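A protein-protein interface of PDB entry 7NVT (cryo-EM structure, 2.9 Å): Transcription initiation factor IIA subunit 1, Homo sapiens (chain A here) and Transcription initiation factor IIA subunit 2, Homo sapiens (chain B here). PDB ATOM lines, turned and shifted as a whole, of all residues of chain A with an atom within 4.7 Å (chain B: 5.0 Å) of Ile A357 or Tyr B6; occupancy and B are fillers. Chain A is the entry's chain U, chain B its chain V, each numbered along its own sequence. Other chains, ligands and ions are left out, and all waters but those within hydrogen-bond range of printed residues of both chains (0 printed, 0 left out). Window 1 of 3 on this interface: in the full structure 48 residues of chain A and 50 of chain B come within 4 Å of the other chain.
O of Val A336 lies within hydrogen-bond range of N of Ile A357, 2.6 Å away.
The side-chain hydroxyl of Thr B9 lies within hydrogen-bond range of the backbone carbonyl oxygen of Tyr B6.
Printed residues of chain B that touch a printed residue of chain A: Leu B5, Tyr B6 and Leu B48.
Among the printed residues, no Asp or Glu carboxylate lies within 4 Å of a Lys or Arg side-chain nitrogen of the other chain.
Ile A357 touches just one residue of chain B: Tyr B6.
Of chain A, only Ile A357 (3.8 Å) comes within 4 Å of Tyr B6.
Of the printed residues of chain B, Val A336 touches Leu B5.
Of the printed residues of chain B, Ile A366 touches Leu B48.
The nearest printed residue of chain A that does not touch Leu B5 is Ile A357 (7.2 Å).
Among the printed residues, merely in contact across the chains: Ile A366 with Leu B48, Ile A357 with Tyr B6, Val A336 with Leu B5 and Cys A337 with Leu B5.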
ATOM      1  N   VAL A 335       1.748 -24.816  -7.149  1.00  0.00           N
ATOM      2  CA  VAL A 335       0.561 -25.420  -7.741  1.00  0.00           C
ATOM      3  C   VAL A 335       0.393 -26.812  -7.150  1.00  0.00           C
ATOM      4  O   VAL A 335       1.327 -27.624  -7.185  1.00  0.00           O
ATOM      5  CB  VAL A 335       0.658 -25.485  -9.274  1.00  0.00           C
ATOM      6  CG1 VAL A 335      -0.458 -26.349  -9.843  1.00  0.00           C
ATOM      7  CG2 VAL A 335       0.611 -24.085  -9.868  1.00  0.00           C
ATOM      8  N   VAL A 336      -0.791 -27.084  -6.611  1.00  0.00           N
ATOM      9  CA  VAL A 336      -1.137 -28.394  -6.073  1.00  0.00           C
ATOM     10  C   VAL A 336      -2.265 -28.969  -6.917  1.00  0.00           C
ATOM     11  O   VAL A 336      -3.291 -28.320  -7.145  1.00  0.00           O
ATOM     12  CB  VAL A 336      -1.545 -28.317  -4.587  1.00  0.00           C
ATOM     13  CG1 VAL A 336      -1.791 -29.709  -4.030  1.00  0.00           C
ATOM     14  CG2 VAL A 336      -0.478 -27.593  -3.779  1.00  0.00           C
ATOM     15  N   CYS A 337      -2.068 -30.199  -7.382  1.00  0.00           N
ATOM     16  CA  CYS A 337      -2.987 -30.807  -8.335  1.00  0.00           C
ATOM     17  C   CYS A 337      -2.899 -32.322  -8.206  1.00  0.00           C
ATOM     18  O   CYS A 337      -2.121 -32.855  -7.411  1.00  0.00           O
ATOM     19  CB  CYS A 337      -2.664 -30.371  -9.766  1.00  0.00           C
ATOM     20  SG  CYS A 337      -1.011 -30.868 -10.310  1.00  0.00           S
ATOM     21  N   GLY A 356      -7.380 -29.371  -9.524  1.00  0.00           N
ATOM     22  CA  GLY A 356      -6.316 -28.947  -8.636  1.00  0.00           C
ATOM     23  C   GLY A 356      -6.490 -27.490  -8.268  1.00  0.00           C
ATOM     24  O   GLY A 356      -7.450 -26.832  -8.675  1.00  0.00           O
ATOM     25  N   ILE A 357      -5.537 -26.988  -7.481  1.00  0.00           N
ATOM     26  CA  ILE A 357      -5.548 -25.610  -7.013  1.00  0.00           C
ATOM     27  C   ILE A 357      -4.193 -24.979  -7.304  1.00  0.00           C
ATOM     28  O   ILE A 357      -3.176 -25.662  -7.438  1.00  0.00           O
ATOM     29  CB  ILE A 357      -5.878 -25.511  -5.507  1.00  0.00           C
ATOM     30  CG1 ILE A 357      -6.329 -24.094  -5.150  1.00  0.00           C
ATOM     31  CG2 ILE A 357      -4.675 -25.917  -4.668  1.00  0.00           C
ATOM     32  CD1 ILE A 357      -7.003 -23.995  -3.797  1.00  0.00           C
ATOM     33  N   MET A 358      -4.195 -23.651  -7.400  1.00  0.00           N
ATOM     34  CA  MET A 358      -2.988 -22.886  -7.675  1.00  0.00           C
ATOM     35  C   MET A 358      -2.991 -21.618  -6.836  1.00  0.00           C
ATOM     36  O   MET A 358      -4.054 -21.114  -6.463  1.00  0.00           O
ATOM     37  CB  MET A 358      -2.880 -22.523  -9.162  1.00  0.00           C
ATOM     38  CG  MET A 358      -3.189 -23.672 -10.108  1.00  0.00           C
ATOM     39  SD  MET A 358      -2.881 -23.253 -11.835  1.00  0.00           S
ATOM     40  CE  MET A 358      -4.363 -22.331 -12.232  1.00  0.00           C
ATOM     41  N   ASN A 359      -1.797 -21.111  -6.543  1.00  0.00           N
ATOM     42  CA  ASN A 359      -1.609 -19.873  -5.788  1.00  0.00           C
ATOM     43  C   ASN A 359      -0.645 -18.999  -6.586  1.00  0.00           C
ATOM     44  O   ASN A 359       0.569 -19.043  -6.375  1.00  0.00           O
ATOM     45  CB  ASN A 359      -1.082 -20.158  -4.381  1.00  0.00           C
ATOM     46  CG  ASN A 359      -1.019 -18.912  -3.519  1.00  0.00           C
ATOM     47  OD1 ASN A 359      -1.406 -17.826  -3.948  1.00  0.00           O
ATOM     48  ND2 ASN A 359      -0.528 -19.065  -2.294  1.00  0.00           N
ATOM     49  N   ASP A 364      -5.757 -16.990  -5.627  1.00  0.00           N
ATOM     50  CA  ASP A 364      -6.048 -18.418  -5.609  1.00  0.00           C
ATOM     51  C   ASP A 364      -6.836 -18.781  -6.861  1.00  0.00           C
ATOM     52  O   ASP A 364      -7.883 -18.184  -7.135  1.00  0.00           O
ATOM     53  CB  ASP A 364      -6.830 -18.797  -4.351  1.00  0.00           C
ATOM     54  CG  ASP A 364      -7.008 -20.295  -4.205  1.00  0.00           C
ATOM     55  OD1 ASP A 364      -5.992 -20.999  -4.027  1.00  0.00           O
ATOM     56  OD2 ASP A 364      -8.161 -20.767  -4.268  1.00  0.00           O
ATOM     57  N   TYR A 365      -6.334 -19.755  -7.612  1.00  0.00           N
ATOM     58  CA  TYR A 365      -6.976 -20.234  -8.826  1.00  0.00           C
ATOM     59  C   TYR A 365      -7.288 -21.719  -8.697  1.00  0.00           C
ATOM     60  O   TYR A 365      -6.478 -22.500  -8.189  1.00  0.00           O
ATOM     61  CB  TYR A 365      -6.088 -19.997 -10.051  1.00  0.00           C
ATOM     62  CG  TYR A 365      -5.969 -18.543 -10.451  1.00  0.00           C
ATOM     63  CD1 TYR A 365      -7.037 -17.874 -11.032  1.00  0.00           C
ATOM     64  CD2 TYR A 365      -4.788 -17.842 -10.250  1.00  0.00           C
ATOM     65  CE1 TYR A 365      -6.934 -16.546 -11.401  1.00  0.00           C
ATOM     66  CE2 TYR A 365      -4.674 -16.514 -10.616  1.00  0.00           C
ATOM     67  CZ  TYR A 365      -5.750 -15.872 -11.190  1.00  0.00           C
ATOM     68  OH  TYR A 365      -5.641 -14.550 -11.555  1.00  0.00           O
ATOM     69  N   ILE A 366      -8.473 -22.102  -9.164  1.00  0.00           N
ATOM     70  CA  ILE A 366      -8.942 -23.480  -9.102  1.00  0.00           C
ATOM     71  C   ILE A 366      -9.353 -23.917 -10.500  1.00  0.00           C
ATOM     72  O   ILE A 366     -10.027 -23.174 -11.223  1.00  0.00           O
ATOM     73  CB  ILE A 366     -10.116 -23.639  -8.111  1.00  0.00           C
ATOM     74  CG1 ILE A 366     -10.282 -25.107  -7.717  1.00  0.00           C
ATOM     75  CG2 ILE A 366     -11.407 -23.097  -8.711  1.00  0.00           C
ATOM     76  CD1 ILE A 366      -9.274 -25.583  -6.695  1.00  0.00           C
ATOM     77  N   PHE A 367      -8.936 -25.122 -10.882  1.00  0.00           N
ATOM     78  CA  PHE A 367      -9.240 -25.683 -12.190  1.00  0.00           C
ATOM     79  C   PHE A 367      -9.680 -27.131 -12.029  1.00  0.00           C
ATOM     80  O   PHE A 367      -9.339 -27.801 -11.052  1.00  0.00           O
ATOM     81  CB  PHE A 367      -8.030 -25.607 -13.131  1.00  0.00           C
ATOM     82  CG  PHE A 367      -6.833 -26.367 -12.637  1.00  0.00           C
ATOM     83  CD1 PHE A 367      -5.956 -25.794 -11.731  1.00  0.00           C
ATOM     84  CD2 PHE A 367      -6.584 -27.656 -13.079  1.00  0.00           C
ATOM     85  CE1 PHE A 367      -4.854 -26.493 -11.275  1.00  0.00           C
ATOM     86  CE2 PHE A 367      -5.484 -28.359 -12.627  1.00  0.00           C
ATOM     87  CZ  PHE A 367      -4.618 -27.776 -11.723  1.00  0.00           C
ATOM     88  N   GLN B   4      -2.954 -35.222   2.526  1.00  0.00           N
ATOM     89  CA  GLN B   4      -2.282 -34.061   3.113  1.00  0.00           C
ATOM     90  C   GLN B   4      -1.528 -33.257   2.049  1.00  0.00           C
ATOM     91  O   GLN B   4      -0.301 -33.144   2.068  1.00  0.00           O
ATOM     92  CB  GLN B   4      -1.338 -34.498   4.238  1.00  0.00           C
ATOM     93  CG  GLN B   4      -1.987 -35.377   5.297  1.00  0.00           C
ATOM     94  CD  GLN B   4      -3.124 -34.682   6.020  1.00  0.00           C
ATOM     95  OE1 GLN B   4      -4.295 -34.980   5.789  1.00  0.00           O
ATOM     96  NE2 GLN B   4      -2.781 -33.754   6.904  1.00  0.00           N
ATOM     97  N   LEU B   5      -2.291 -32.695   1.111  1.00  0.00           N
ATOM     98  CA  LEU B   5      -1.732 -31.886   0.032  1.00  0.00           C
ATOM     99  C   LEU B   5      -1.873 -30.388   0.274  1.00  0.00           C
ATOM    100  O   LEU B   5      -0.884 -29.653   0.191  1.00  0.00           O
ATOM    101  CB  LEU B   5      -2.398 -32.249  -1.301  1.00  0.00           C
ATOM    102  CG  LEU B   5      -1.732 -33.372  -2.095  1.00  0.00           C
ATOM    103  CD1 LEU B   5      -1.922 -34.697  -1.391  1.00  0.00           C
ATOM    104  CD2 LEU B   5      -2.287 -33.426  -3.508  1.00  0.00           C
ATOM    105  N   TYR B   6      -3.081 -29.917   0.572  1.00  0.00           N
ATOM    106  CA  TYR B   6      -3.368 -28.491   0.639  1.00  0.00           C
ATOM    107  C   TYR B   6      -2.983 -27.863   1.973  1.00  0.00           C
ATOM    108  O   TYR B   6      -3.305 -26.693   2.206  1.00  0.00           O
ATOM    109  CB  TYR B   6      -4.853 -28.242   0.361  1.00  0.00           C
ATOM    110  CG  TYR B   6      -5.399 -29.051  -0.795  1.00  0.00           C
ATOM    111  CD1 TYR B   6      -5.263 -28.606  -2.103  1.00  0.00           C
ATOM    112  CD2 TYR B   6      -6.053 -30.256  -0.578  1.00  0.00           C
ATOM    113  CE1 TYR B   6      -5.759 -29.341  -3.162  1.00  0.00           C
ATOM    114  CE2 TYR B   6      -6.552 -30.998  -1.631  1.00  0.00           C
ATOM    115  CZ  TYR B   6      -6.402 -30.535  -2.921  1.00  0.00           C
ATOM    116  OH  TYR B   6      -6.899 -31.270  -3.973  1.00  0.00           O
ATOM    117  N   ARG B   7      -2.308 -28.605   2.852  1.00  0.00           N
ATOM    118  CA  ARG B   7      -1.873 -28.024   4.118  1.00  0.00           C
ATOM    119  C   ARG B   7      -0.880 -26.891   3.893  1.00  0.00           C
ATOM    120  O   ARG B   7      -0.950 -25.852   4.559  1.00  0.00           O
ATOM    121  CB  ARG B   7      -1.258 -29.104   5.007  1.00  0.00           C
ATOM    122  CG  ARG B   7      -2.282 -29.966   5.734  1.00  0.00           C
ATOM    123  CD  ARG B   7      -1.655 -30.750   6.879  1.00  0.00           C
ATOM    124  NE  ARG B   7      -0.963 -29.887   7.834  1.00  0.00           N
ATOM    125  CZ  ARG B   7      -0.280 -30.329   8.885  1.00  0.00           C
ATOM    126  NH1 ARG B   7      -0.189 -31.631   9.126  1.00  0.00           N
ATOM    127  NH2 ARG B   7       0.317 -29.468   9.697  1.00  0.00           N
ATOM    128  N   ASN B   8       0.052 -27.070   2.958  1.00  0.00           N
ATOM    129  CA  ASN B   8       1.079 -26.066   2.679  1.00  0.00           C
ATOM    130  C   ASN B   8       0.568 -25.043   1.664  1.00  0.00           C
ATOM    131  O   ASN B   8       1.119 -24.860   0.578  1.00  0.00           O
ATOM    132  CB  ASN B   8       2.356 -26.743   2.191  1.00  0.00           C
ATOM    133  CG  ASN B   8       3.548 -25.806   2.189  1.00  0.00           C
ATOM    134  OD1 ASN B   8       3.808 -25.115   1.203  1.00  0.00           O
ATOM    135  ND2 ASN B   8       4.278 -25.776   3.298  1.00  0.00           N
ATOM    136  N   THR B   9      -0.515 -24.368   2.044  1.00  0.00           N
ATOM    137  CA  THR B   9      -1.123 -23.329   1.225  1.00  0.00           C
ATOM    138  C   THR B   9      -1.596 -22.206   2.139  1.00  0.00           C
ATOM    139  O   THR B   9      -1.566 -22.322   3.368  1.00  0.00           O
ATOM    140  CB  THR B   9      -2.285 -23.880   0.390  1.00  0.00           C
ATOM    141  OG1 THR B   9      -3.342 -24.308   1.257  1.00  0.00           O
ATOM    142  CG2 THR B   9      -1.826 -25.049  -0.469  1.00  0.00           C
ATOM    143  N   GLY B  12      -4.454 -23.528   4.054  1.00  0.00           N
ATOM    144  CA  GLY B  12      -3.954 -24.429   5.079  1.00  0.00           C
ATOM    145  C   GLY B  12      -3.177 -23.704   6.161  1.00  0.00           C
ATOM    146  O   GLY B  12      -3.308 -24.016   7.348  1.00  0.00           O
ATOM    147  N   ASP B  41      -8.911 -31.634   5.498  1.00  0.00           N
ATOM    148  CA  ASP B  41      -8.328 -32.180   4.277  1.00  0.00           C
ATOM    149  C   ASP B  41      -9.343 -33.018   3.511  1.00  0.00           C
ATOM    150  O   ASP B  41      -9.409 -32.955   2.278  1.00  0.00           O
ATOM    151  CB  ASP B  41      -7.090 -33.009   4.617  1.00  0.00           C
ATOM    152  CG  ASP B  41      -5.889 -32.149   4.963  1.00  0.00           C
ATOM    153  OD1 ASP B  41      -5.713 -31.087   4.328  1.00  0.00           O
ATOM    154  OD2 ASP B  41      -5.124 -32.528   5.873  1.00  0.00           O
ATOM    155  N   ILE B  44     -11.950 -30.472   1.893  1.00  0.00           N
ATOM    156  CA  ILE B  44     -11.434 -29.732   0.745  1.00  0.00           C
ATOM    157  C   ILE B  44     -11.213 -30.667  -0.437  1.00  0.00           C
ATOM    158  O   ILE B  44     -11.494 -30.311  -1.588  1.00  0.00           O
ATOM    159  CB  ILE B  44     -10.145 -28.980   1.126  1.00  0.00           C
ATOM    160  CG1 ILE B  44      -9.705 -28.066  -0.019  1.00  0.00           C
ATOM    161  CG2 ILE B  44      -9.030 -29.954   1.476  1.00  0.00           C
ATOM    162  CD1 ILE B  44      -8.770 -26.959   0.412  1.00  0.00           C
ATOM    163  N   ASN B  45     -10.707 -31.875  -0.178  1.00  0.00           N
ATOM    164  CA  ASN B  45     -10.476 -32.825  -1.263  1.00  0.00           C
ATOM    165  C   ASN B  45     -11.782 -33.176  -1.964  1.00  0.00           C
ATOM    166  O   ASN B  45     -11.844 -33.230  -3.197  1.00  0.00           O
ATOM    167  CB  ASN B  45      -9.801 -34.085  -0.718  1.00  0.00           C
ATOM    168  CG  ASN B  45      -8.289 -34.019  -0.805  1.00  0.00           C
ATOM    169  OD1 ASN B  45      -7.707 -34.225  -1.870  1.00  0.00           O
ATOM    170  ND2 ASN B  45      -7.644 -33.733   0.320  1.00  0.00           N
ATOM    171  N   LEU B  48     -13.145 -29.985  -3.985  1.00  0.00           N
ATOM    172  CA  LEU B  48     -12.470 -29.709  -5.249  1.00  0.00           C
ATOM    173  C   LEU B  48     -12.919 -30.673  -6.339  1.00  0.00           C
ATOM    174  O   LEU B  48     -13.137 -30.268  -7.487  1.00  0.00           O
ATOM    175  CB  LEU B  48     -10.955 -29.785  -5.063  1.00  0.00           C
ATOM    176  CG  LEU B  48     -10.257 -28.451  -4.795  1.00  0.00           C
ATOM    177  CD1 LEU B  48     -10.611 -27.920  -3.416  1.00  0.00           C
ATOM    178  CD2 LEU B  48      -8.750 -28.600  -4.945  1.00  0.00           C
